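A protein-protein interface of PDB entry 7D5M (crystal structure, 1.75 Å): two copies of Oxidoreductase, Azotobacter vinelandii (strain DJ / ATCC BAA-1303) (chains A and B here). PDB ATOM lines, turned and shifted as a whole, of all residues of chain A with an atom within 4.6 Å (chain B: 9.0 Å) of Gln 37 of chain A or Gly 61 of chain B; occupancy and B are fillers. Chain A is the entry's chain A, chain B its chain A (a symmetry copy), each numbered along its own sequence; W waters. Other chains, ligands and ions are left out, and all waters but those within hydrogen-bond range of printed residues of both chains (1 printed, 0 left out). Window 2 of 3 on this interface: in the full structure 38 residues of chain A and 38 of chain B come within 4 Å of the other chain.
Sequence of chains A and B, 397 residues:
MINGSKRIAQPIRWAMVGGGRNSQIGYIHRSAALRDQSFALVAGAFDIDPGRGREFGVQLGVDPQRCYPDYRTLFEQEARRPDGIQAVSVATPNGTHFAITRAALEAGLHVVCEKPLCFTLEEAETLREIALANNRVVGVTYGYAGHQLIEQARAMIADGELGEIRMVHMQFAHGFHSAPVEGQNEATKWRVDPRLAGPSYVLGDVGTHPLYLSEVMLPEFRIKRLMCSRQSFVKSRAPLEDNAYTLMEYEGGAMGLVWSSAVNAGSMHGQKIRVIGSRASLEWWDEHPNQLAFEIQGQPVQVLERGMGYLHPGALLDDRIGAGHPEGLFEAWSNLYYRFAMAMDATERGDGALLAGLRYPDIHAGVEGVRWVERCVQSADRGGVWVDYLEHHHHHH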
ATOM      1  N   GLY A   4      13.944 -19.316 -15.758  1.00  0.00           N
ATOM      2  CA  GLY A   4      14.899 -19.373 -16.881  1.00  0.00           C
ATOM      3  C   GLY A   4      15.336 -20.789 -17.213  1.00  0.00           C
ATOM      4  O   GLY A   4      16.164 -20.961 -18.125  1.00  0.00           O
ATOM      5  N   SER A   5      14.810 -21.785 -16.507  1.00  0.00           N
ATOM      6  CA  SER A   5      15.108 -23.212 -16.765  1.00  0.00           C
ATOM      7  C   SER A   5      14.616 -23.549 -18.176  1.00  0.00           C
ATOM      8  O   SER A   5      13.565 -22.996 -18.611  1.00  0.00           O
ATOM      9  CB  SER A   5      14.499 -24.083 -15.706  1.00  0.00           C
ATOM     10  OG  SER A   5      13.092 -24.014 -15.780  1.00  0.00           O
ATOM     11  N   LYS A   6      15.336 -24.408 -18.892  1.00  0.00           N
ATOM     12  CA  LYS A   6      14.954 -24.728 -20.288  1.00  0.00           C
ATOM     13  C   LYS A   6      13.590 -25.429 -20.297  1.00  0.00           C
ATOM     14  O   LYS A   6      13.266 -26.180 -19.363  1.00  0.00           O
ATOM     15  CB  LYS A   6      16.039 -25.537 -20.995  1.00  0.00           C
ATOM     16  CG  LYS A   6      16.283 -26.935 -20.463  1.00  0.00           C
ATOM     17  CD  LYS A   6      17.335 -27.678 -21.284  1.00  0.00           C
ATOM     18  CE  LYS A   6      18.711 -27.059 -21.194  1.00  0.00           C
ATOM     19  NZ  LYS A   6      19.611 -27.579 -22.249  1.00  0.00           N
ATOM     20  N   ILE A   8      12.580 -26.760 -23.491  1.00  0.00           N
ATOM     21  CA  ILE A   8      12.890 -27.727 -24.574  1.00  0.00           C
ATOM     22  C   ILE A   8      14.385 -28.017 -24.457  1.00  0.00           C
ATOM     23  O   ILE A   8      15.089 -27.185 -23.846  1.00  0.00           O
ATOM     24  CB  ILE A   8      12.466 -27.158 -25.945  1.00  0.00           C
ATOM     25  CG1 ILE A   8      13.251 -25.898 -26.322  1.00  0.00           C
ATOM     26  CG2 ILE A   8      10.966 -26.885 -25.958  1.00  0.00           C
ATOM     27  CD1 ILE A   8      12.987 -25.414 -27.728  1.00  0.00           C
ATOM     28  N   PRO A  11      17.671 -24.828 -27.864  1.00  0.00           N
ATOM     29  CA  PRO A  11      16.993 -23.710 -28.512  1.00  0.00           C
ATOM     30  C   PRO A  11      16.698 -24.036 -29.979  1.00  0.00           C
ATOM     31  O   PRO A  11      17.541 -24.652 -30.647  1.00  0.00           O
ATOM     32  CB  PRO A  11      17.990 -22.550 -28.385  1.00  0.00           C
ATOM     33  CG  PRO A  11      18.832 -22.938 -27.192  1.00  0.00           C
ATOM     34  CD  PRO A  11      18.985 -24.435 -27.335  1.00  0.00           C
ATOM     35  N   LEU A  34      15.027 -14.948 -27.835  1.00  0.00           N
ATOM     36  CA  LEU A  34      16.353 -15.379 -27.320  1.00  0.00           C
ATOM     37  C   LEU A  34      16.265 -15.637 -25.815  1.00  0.00           C
ATOM     38  O   LEU A  34      17.130 -16.342 -25.268  1.00  0.00           O
ATOM     39  CB  LEU A  34      17.387 -14.313 -27.669  1.00  0.00           C
ATOM     40  CG  LEU A  34      17.586 -14.073 -29.164  1.00  0.00           C
ATOM     41  CD1 LEU A  34      18.550 -12.925 -29.382  1.00  0.00           C
ATOM     42  CD2 LEU A  34      18.084 -15.329 -29.865  1.00  0.00           C
ATOM     43  N   ARG A  35      15.228 -15.117 -25.175  1.00  0.00           N
ATOM     44  CA  ARG A  35      15.059 -15.218 -23.712  1.00  0.00           C
ATOM     45  C   ARG A  35      14.861 -16.681 -23.309  1.00  0.00           C
ATOM     46  O   ARG A  35      14.159 -17.428 -24.033  1.00  0.00           O
ATOM     47  CB  ARG A  35      13.879 -14.363 -23.264  1.00  0.00           C
ATOM     48  CG  ARG A  35      13.905 -14.046 -21.779  1.00  0.00           C
ATOM     49  CD  ARG A  35      12.727 -13.153 -21.471  1.00  0.00           C
ATOM     50  NE  ARG A  35      12.817 -12.530 -20.166  1.00  0.00           N
ATOM     51  CZ  ARG A  35      12.002 -11.573 -19.743  1.00  0.00           C
ATOM     52  NH1 ARG A  35      10.993 -11.187 -20.503  1.00  0.00           N
ATOM     53  NH2 ARG A  35      12.153 -11.062 -18.534  1.00  0.00           N
ATOM     54  N   ASP A  36      15.486 -17.087 -22.199  1.00  0.00           N
ATOM     55  CA  ASP A  36      15.195 -18.383 -21.527  1.00  0.00           C
ATOM     56  C   ASP A  36      15.483 -19.563 -22.462  1.00  0.00           C
ATOM     57  O   ASP A  36      14.794 -20.588 -22.347  1.00  0.00           O
ATOM     58  CB  ASP A  36      13.745 -18.460 -21.044  1.00  0.00           C
ATOM     59  CG  ASP A  36      13.325 -17.285 -20.185  1.00  0.00           C
ATOM     60  OD1 ASP A  36      14.198 -16.724 -19.498  1.00  0.00           O
ATOM     61  OD2 ASP A  36      12.122 -16.937 -20.216  1.00  0.00           O
ATOM     62  N   GLN A  37      16.458 -19.423 -23.353  1.00  0.00           N
ATOM     63  CA  GLN A  37      16.969 -20.550 -24.173  1.00  0.00           C
ATOM     64  C   GLN A  37      15.867 -21.060 -25.119  1.00  0.00           C
ATOM     65  O   GLN A  37      15.880 -22.274 -25.419  1.00  0.00           O
ATOM     66  CB  GLN A  37      17.449 -21.693 -23.265  1.00  0.00           C
ATOM     67  CG  GLN A  37      18.339 -21.256 -22.102  1.00  0.00           C
ATOM     68  CD  GLN A  37      18.767 -22.425 -21.244  1.00  0.00           C
ATOM     69  OE1 GLN A  37      19.643 -23.198 -21.619  1.00  0.00           O
ATOM     70  NE2 GLN A  37      18.138 -22.575 -20.086  1.00  0.00           N
ATOM     71  N   SER A  38      14.938 -20.212 -25.585  1.00  0.00           N
ATOM     72  CA  SER A  38      13.821 -20.657 -26.469  1.00  0.00           C
ATOM     73  C   SER A  38      14.318 -20.852 -27.906  1.00  0.00           C
ATOM     74  O   SER A  38      14.107 -21.950 -28.492  1.00  0.00           O
ATOM     75  CB  SER A  38      12.655 -19.696 -26.433  1.00  0.00           C
ATOM     76  OG  SER A  38      11.983 -19.777 -25.181  1.00  0.00           O
ATOM     77  N   PHE A  39      14.939 -19.816 -28.459  1.00  0.00           N
ATOM     78  CA  PHE A  39      15.459 -19.766 -29.846  1.00  0.00           C
ATOM     79  C   PHE A  39      16.914 -19.297 -29.819  1.00  0.00           C
ATOM     80  O   PHE A  39      17.319 -18.565 -28.882  1.00  0.00           O
ATOM     81  CB  PHE A  39      14.628 -18.811 -30.712  1.00  0.00           C
ATOM     82  CG  PHE A  39      13.203 -19.228 -30.935  1.00  0.00           C
ATOM     83  CD1 PHE A  39      12.237 -19.006 -29.970  1.00  0.00           C
ATOM     84  CD2 PHE A  39      12.831 -19.873 -32.105  1.00  0.00           C
ATOM     85  CE1 PHE A  39      10.928 -19.403 -30.182  1.00  0.00           C
ATOM     86  CE2 PHE A  39      11.514 -20.255 -32.319  1.00  0.00           C
ATOM     87  CZ  PHE A  39      10.568 -20.033 -31.349  1.00  0.00           C
ATOM     88  N   TYR B  27      16.479 -14.821 -11.097  1.00  0.00           N
ATOM     89  CA  TYR B  27      16.037 -14.779 -12.511  1.00  0.00           C
ATOM     90  C   TYR B  27      16.277 -13.394 -13.128  1.00  0.00           C
ATOM     91  O   TYR B  27      16.779 -13.313 -14.265  1.00  0.00           O
ATOM     92  CB  TYR B  27      14.574 -15.188 -12.671  1.00  0.00           C
ATOM     93  CG  TYR B  27      14.155 -15.076 -14.111  1.00  0.00           C
ATOM     94  CD1 TYR B  27      14.706 -15.916 -15.064  1.00  0.00           C
ATOM     95  CD2 TYR B  27      13.325 -14.055 -14.539  1.00  0.00           C
ATOM     96  CE1 TYR B  27      14.389 -15.790 -16.403  1.00  0.00           C
ATOM     97  CE2 TYR B  27      12.990 -13.924 -15.877  1.00  0.00           C
ATOM     98  CZ  TYR B  27      13.525 -14.790 -16.812  1.00  0.00           C
ATOM     99  OH  TYR B  27      13.215 -14.660 -18.133  1.00  0.00           O
ATOM    100  N   ARG B  30      19.795 -12.825 -14.338  1.00  0.00           N
ATOM    101  CA  ARG B  30      20.111 -13.551 -15.594  1.00  0.00           C
ATOM    102  C   ARG B  30      19.371 -12.896 -16.764  1.00  0.00           C
ATOM    103  O   ARG B  30      19.964 -12.759 -17.837  1.00  0.00           O
ATOM    104  CB  ARG B  30      19.767 -15.030 -15.467  1.00  0.00           C
ATOM    105  CG  ARG B  30      20.672 -15.770 -14.494  1.00  0.00           C
ATOM    106  CD  ARG B  30      20.397 -17.268 -14.487  1.00  0.00           C
ATOM    107  NE  ARG B  30      19.059 -17.605 -14.018  1.00  0.00           N
ATOM    108  CZ  ARG B  30      18.714 -17.755 -12.740  1.00  0.00           C
ATOM    109  NH1 ARG B  30      19.607 -17.577 -11.783  1.00  0.00           N
ATOM    110  NH2 ARG B  30      17.469 -18.063 -12.422  1.00  0.00           N
ATOM    111  N   LEU B  34      22.008 -11.547 -19.571  1.00  0.00           N
ATOM    112  CA  LEU B  34      22.144 -12.356 -20.810  1.00  0.00           C
ATOM    113  C   LEU B  34      21.606 -11.566 -22.006  1.00  0.00           C
ATOM    114  O   LEU B  34      21.954 -11.890 -23.153  1.00  0.00           O
ATOM    115  CB  LEU B  34      21.418 -13.682 -20.614  1.00  0.00           C
ATOM    116  CG  LEU B  34      21.969 -14.558 -19.491  1.00  0.00           C
ATOM    117  CD1 LEU B  34      21.106 -15.792 -19.323  1.00  0.00           C
ATOM    118  CD2 LEU B  34      23.416 -14.951 -19.754  1.00  0.00           C
ATOM    119  N   ALA B  40      27.667 -13.847 -20.682  1.00  0.00           N
ATOM    120  CA  ALA B  40      27.408 -15.277 -20.942  1.00  0.00           C
ATOM    121  C   ALA B  40      27.567 -16.041 -19.626  1.00  0.00           C
ATOM    122  O   ALA B  40      28.660 -15.967 -19.025  1.00  0.00           O
ATOM    123  CB  ALA B  40      28.351 -15.795 -22.000  1.00  0.00           C
ATOM    124  N   LEU B  41      26.523 -16.758 -19.217  1.00  0.00           N
ATOM    125  CA  LEU B  41      26.520 -17.559 -17.973  1.00  0.00           C
ATOM    126  C   LEU B  41      27.205 -18.899 -18.248  1.00  0.00           C
ATOM    127  O   LEU B  41      26.583 -19.790 -18.883  1.00  0.00           O
ATOM    128  CB  LEU B  41      25.088 -17.769 -17.482  1.00  0.00           C
ATOM    129  CG  LEU B  41      24.965 -18.561 -16.182  1.00  0.00           C
ATOM    130  CD1 LEU B  41      25.622 -17.810 -15.037  1.00  0.00           C
ATOM    131  CD2 LEU B  41      23.511 -18.864 -15.874  1.00  0.00           C
ATOM    132  N   VAL B  42      28.443 -19.033 -17.783  1.00  0.00           N
ATOM    133  CA  VAL B  42      29.298 -20.218 -18.098  1.00  0.00           C
ATOM    134  C   VAL B  42      29.586 -21.021 -16.829  1.00  0.00           C
ATOM    135  O   VAL B  42      30.130 -22.127 -16.967  1.00  0.00           O
ATOM    136  CB  VAL B  42      30.591 -19.792 -18.816  1.00  0.00           C
ATOM    137  CG1 VAL B  42      30.265 -19.113 -20.133  1.00  0.00           C
ATOM    138  CG2 VAL B  42      31.471 -18.903 -17.949  1.00  0.00           C
ATOM    139  N   ALA B  43      29.225 -20.521 -15.646  1.00  0.00           N
ATOM    140  CA  ALA B  43      29.563 -21.183 -14.364  1.00  0.00           C
ATOM    141  C   ALA B  43      28.706 -20.613 -13.234  1.00  0.00           C
ATOM    142  O   ALA B  43      28.078 -19.571 -13.422  1.00  0.00           O
ATOM    143  CB  ALA B  43      31.029 -21.001 -14.061  1.00  0.00           C
ATOM    144  N   PHE B  46      25.236 -21.886  -7.352  1.00  0.00           N
ATOM    145  CA  PHE B  46      23.854 -21.352  -7.442  1.00  0.00           C
ATOM    146  C   PHE B  46      23.077 -21.512  -6.132  1.00  0.00           C
ATOM    147  O   PHE B  46      22.104 -20.774  -5.953  1.00  0.00           O
ATOM    148  CB  PHE B  46      23.099 -22.032  -8.582  1.00  0.00           C
ATOM    149  CG  PHE B  46      23.589 -21.639  -9.950  1.00  0.00           C
ATOM    150  CD1 PHE B  46      23.357 -20.358 -10.435  1.00  0.00           C
ATOM    151  CD2 PHE B  46      24.322 -22.521 -10.726  1.00  0.00           C
ATOM    152  CE1 PHE B  46      23.823 -19.986 -11.688  1.00  0.00           C
ATOM    153  CE2 PHE B  46      24.793 -22.146 -11.977  1.00  0.00           C
ATOM    154  CZ  PHE B  46      24.537 -20.881 -12.458  1.00  0.00           C
ATOM    155  N   ARG B  54      23.560 -27.665  -8.787  1.00  0.00           N
ATOM    156  CA  ARG B  54      24.039 -28.302 -10.037  1.00  0.00           C
ATOM    157  C   ARG B  54      22.835 -28.698 -10.901  1.00  0.00           C
ATOM    158  O   ARG B  54      22.888 -28.460 -12.119  1.00  0.00           O
ATOM    159  CB  ARG B  54      24.930 -29.514  -9.754  1.00  0.00           C
ATOM    160  CG  ARG B  54      25.426 -30.191 -11.022  1.00  0.00           C
ATOM    161  CD  ARG B  54      26.524 -31.212 -10.797  1.00  0.00           C
ATOM    162  NE  ARG B  54      27.772 -30.578 -10.388  1.00  0.00           N
ATOM    163  CZ  ARG B  54      28.324 -30.667  -9.176  1.00  0.00           C
ATOM    164  NH1 ARG B  54      27.753 -31.373  -8.211  1.00  0.00           N
ATOM    165  NH2 ARG B  54      29.459 -30.035  -8.935  1.00  0.00           N
ATOM    166  N   GLU B  55      21.799 -29.300 -10.311  1.00  0.00           N
ATOM    167  CA  GLU B  55      20.552 -29.635 -11.050  1.00  0.00           C
ATOM    168  C   GLU B  55      20.068 -28.386 -11.791  1.00  0.00           C
ATOM    169  O   GLU B  55      19.727 -28.489 -12.987  1.00  0.00           O
ATOM    170  CB  GLU B  55      19.433 -30.095 -10.119  1.00  0.00           C
ATOM    171  CG  GLU B  55      19.604 -31.502  -9.598  1.00  0.00           C
ATOM    172  CD  GLU B  55      18.591 -31.853  -8.522  1.00  0.00           C
ATOM    173  OE1 GLU B  55      17.547 -31.166  -8.438  1.00  0.00           O
ATOM    174  OE2 GLU B  55      18.852 -32.793  -7.759  1.00  0.00           O
ATOM    175  N   PHE B  56      20.018 -27.252 -11.095  1.00  0.00           N
ATOM    176  CA  PHE B  56      19.454 -25.989 -11.642  1.00  0.00           C
ATOM    177  C   PHE B  56      20.412 -25.416 -12.695  1.00  0.00           C
ATOM    178  O   PHE B  56      19.949 -25.028 -13.788  1.00  0.00           O
ATOM    179  CB  PHE B  56      19.148 -24.986 -10.525  1.00  0.00           C
ATOM    180  CG  PHE B  56      18.457 -23.736 -11.007  1.00  0.00           C
ATOM    181  CD1 PHE B  56      17.270 -23.820 -11.720  1.00  0.00           C
ATOM    182  CD2 PHE B  56      18.976 -22.481 -10.732  1.00  0.00           C
ATOM    183  CE1 PHE B  56      16.635 -22.671 -12.167  1.00  0.00           C
ATOM    184  CE2 PHE B  56      18.327 -21.336 -11.163  1.00  0.00           C
ATOM    185  CZ  PHE B  56      17.163 -21.436 -11.885  1.00  0.00           C
ATOM    186  N   GLY B  57      21.714 -25.349 -12.389  1.00  0.00           N
ATOM    187  CA  GLY B  57      22.737 -24.882 -13.346  1.00  0.00           C
ATOM    188  C   GLY B  57      22.597 -25.600 -14.681  1.00  0.00           C
ATOM    189  O   GLY B  57      22.606 -24.921 -15.735  1.00  0.00           O
ATOM    190  N   VAL B  58      22.396 -26.918 -14.645  1.00  0.00           N
ATOM    191  CA  VAL B  58      22.253 -27.743 -15.884  1.00  0.00           C
ATOM    192  C   VAL B  58      20.991 -27.297 -16.632  1.00  0.00           C
ATOM    193  O   VAL B  58      21.075 -27.149 -17.880  1.00  0.00           O
ATOM    194  CB  VAL B  58      22.256 -29.253 -15.585  1.00  0.00           C
ATOM    195  CG1 VAL B  58      21.792 -30.076 -16.783  1.00  0.00           C
ATOM    196  CG2 VAL B  58      23.641 -29.696 -15.128  1.00  0.00           C
ATOM    197  N   GLN B  59      19.899 -27.008 -15.918  1.00  0.00           N
ATOM    198  CA  GLN B  59      18.635 -26.548 -16.558  1.00  0.00           C
ATOM    199  C   GLN B  59      18.816 -25.127 -17.111  1.00  0.00           C
ATOM    200  O   GLN B  59      18.043 -24.750 -18.024  1.00  0.00           O
ATOM    201  CB  GLN B  59      17.453 -26.702 -15.599  1.00  0.00           C
ATOM    202  CG  GLN B  59      17.095 -28.158 -15.304  1.00  0.00           C
ATOM    203  CD  GLN B  59      17.131 -29.064 -16.520  1.00  0.00           C
ATOM    204  OE1 GLN B  59      16.464 -28.820 -17.528  1.00  0.00           O
ATOM    205  NE2 GLN B  59      17.918 -30.132 -16.445  1.00  0.00           N
ATOM    206  N   LEU B  60      19.800 -24.373 -16.608  1.00  0.00           N
ATOM    207  CA  LEU B  60      20.186 -23.040 -17.142  1.00  0.00           C
ATOM    208  C   LEU B  60      21.180 -23.168 -18.300  1.00  0.00           C
ATOM    209  O   LEU B  60      21.570 -22.107 -18.838  1.00  0.00           O
ATOM    210  CB  LEU B  60      20.787 -22.180 -16.027  1.00  0.00           C
ATOM    211  CG  LEU B  60      19.832 -21.723 -14.930  1.00  0.00           C
ATOM    212  CD1 LEU B  60      20.577 -20.894 -13.894  1.00  0.00           C
ATOM    213  CD2 LEU B  60      18.662 -20.925 -15.494  1.00  0.00           C
ATOM    214  N   GLY B  61      21.588 -24.389 -18.666  1.00  0.00           N
ATOM    215  CA  GLY B  61      22.491 -24.659 -19.802  1.00  0.00           C
ATOM    216  C   GLY B  61      23.961 -24.578 -19.417  1.00  0.00           C
ATOM    217  O   GLY B  61      24.806 -24.539 -20.327  1.00  0.00           O
ATOM    218  N   VAL B  62      24.276 -24.590 -18.119  1.00  0.00           N
ATOM    219  CA  VAL B  62      25.675 -24.525 -17.604  1.00  0.00           C
ATOM    220  C   VAL B  62      26.262 -25.940 -17.574  1.00  0.00           C
ATOM    221  O   VAL B  62      25.550 -26.875 -17.198  1.00  0.00           O
ATOM    222  CB  VAL B  62      25.742 -23.856 -16.220  1.00  0.00           C
ATOM    223  CG1 VAL B  62      27.169 -23.749 -15.701  1.00  0.00           C
ATOM    224  CG2 VAL B  62      25.088 -22.484 -16.249  1.00  0.00           C
ATOM    225  N   ASP B  63      27.525 -26.063 -17.970  1.00  0.00           N
ATOM    226  CA  ASP B  63      28.322 -27.308 -17.865  1.00  0.00           C
ATOM    227  C   ASP B  63      28.250 -27.790 -16.421  1.00  0.00           C
ATOM    228  O   ASP B  63      28.622 -27.031 -15.531  1.00  0.00           O
ATOM    229  CB  ASP B  63      29.758 -27.014 -18.288  1.00  0.00           C
ATOM    230  CG  ASP B  63      30.689 -28.210 -18.301  1.00  0.00           C
ATOM    231  OD1 ASP B  63      30.354 -29.235 -17.680  1.00  0.00           O
ATOM    232  OD2 ASP B  63      31.732 -28.091 -18.940  1.00  0.00           O
ATOM    233  N   PRO B  64      27.791 -29.035 -16.131  1.00  0.00           N
ATOM    234  CA  PRO B  64      27.684 -29.513 -14.749  1.00  0.00           C
ATOM    235  C   PRO B  64      29.015 -29.426 -13.984  1.00  0.00           C
ATOM    236  O   PRO B  64      29.006 -29.208 -12.777  1.00  0.00           O
ATOM    237  CB  PRO B  64      27.226 -30.981 -14.881  1.00  0.00           C
ATOM    238  CG  PRO B  64      27.547 -31.346 -16.310  1.00  0.00           C
ATOM    239  CD  PRO B  64      27.367 -30.065 -17.099  1.00  0.00           C
ATOM    240  N   ARG B  66      31.057 -27.049 -14.234  1.00  0.00           N
ATOM    241  CA  ARG B  66      31.263 -25.619 -13.874  1.00  0.00           C
ATOM    242  C   ARG B  66      30.126 -25.141 -12.963  1.00  0.00           C
ATOM    243  O   ARG B  66      29.991 -23.918 -12.784  1.00  0.00           O
ATOM    244  CB  ARG B  66      31.375 -24.757 -15.134  1.00  0.00           C
ATOM    245  CG  ARG B  66      32.538 -25.141 -16.033  1.00  0.00           C
ATOM    246  CD  ARG B  66      32.617 -24.264 -17.259  1.00  0.00           C
ATOM    247  NE  ARG B  66      33.402 -23.052 -17.057  1.00  0.00           N
ATOM    248  CZ  ARG B  66      33.662 -22.168 -18.016  1.00  0.00           C
ATOM    249  NH1 ARG B  66      33.196 -22.371 -19.236  1.00  0.00           N
ATOM    250  NH2 ARG B  66      34.376 -21.085 -17.762  1.00  0.00           N
ATOM    251  N   CYS B  67      29.339 -26.069 -12.421  1.00  0.00           N
ATOM    252  CA  CYS B  67      28.423 -25.830 -11.279  1.00  0.00           C
ATOM    253  C   CYS B  67      29.169 -26.259 -10.018  1.00  0.00           C
ATOM    254  O   CYS B  67      29.185 -27.469  -9.720  1.00  0.00           O
ATOM    255  CB  CYS B  67      27.116 -26.597 -11.401  1.00  0.00           C
ATOM    256  SG  CYS B  67      26.178 -26.175 -12.893  1.00  0.00           S
HETATM  257  O   HOH W   1      14.483 -27.394 -17.284  1.00  0.00           O
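The backbone carbonyl oxygen (O) of Gln 59 of chain B lies within hydrogen-bond range of the backbone NH (N) of Lys 6 of chain A, 2.9 Å away.
OH of Tyr 27 of chain B lies within hydrogen-bond range of NE of Arg 35 of chain A, at 3.0 Å.
O of Gln 59 of chain B is in hydrogen-bond range of NE2 of Gln 37 of chain A (3.0 Å).
OH of Tyr 27 of chain B is in hydrogen-bond range of OD1 of Asp 36 of chain A.
O of Gly 4 of chain A is in hydrogen-bond range of NE2 of Gln 37 of chain A, 3.2 Å away.
O of Arg 35 of chain A sits at hydrogen-bond distance from OG of Ser 38 of chain A.
Among the printed residues, merely in contact across the chains: Gly 4 of chain A with Tyr 27 of chain B (3.6 Å), Gly 4 of chain A with Leu 60 of chain B (3.6 Å), Ser 5 of chain A with Gln 59 of chain B (3.5 Å), Gln 37 of chain A with Leu 60 of chain B (3.6 Å) and Gln 37 of chain A with Gly 61 of chain B (3.7 Å).
Gly 61 of chain B touches one residue of chain A.
No residue of chain B comes within 4 Å of Ser 38 of chain A.
Of the printed residues of chain B, Gly 4 of chain A touches Tyr 27 (3.6 Å) and Leu 60 (3.6 Å).
Of the printed residues of chain B, Arg 35 of chain A touches Tyr 27 (3.0 Å).
The nearest residue of chain B that does not touch Gln 37 of chain A is Val 58 of chain B (5.6 Å).
The nearest printed residue of chain B that does not touch Gly 4 of chain A is Gln 59 of chain B (4.2 Å).
Printed residues of chain A that touch a printed residue of chain B: Gly 4, Ser 5, Lys 6, Arg 35, Asp 36 and Gln 37.
Among the printed residues, 9 pairs touch across the chains.
1 position is printed for both chains.
Water W1 bridges the side-chain amide oxygen (OE1) of Gln 59 of chain B (2.5 Å) and the backbone carbonyl oxygen (O) of Lys 6 of chain A (2.7 Å).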
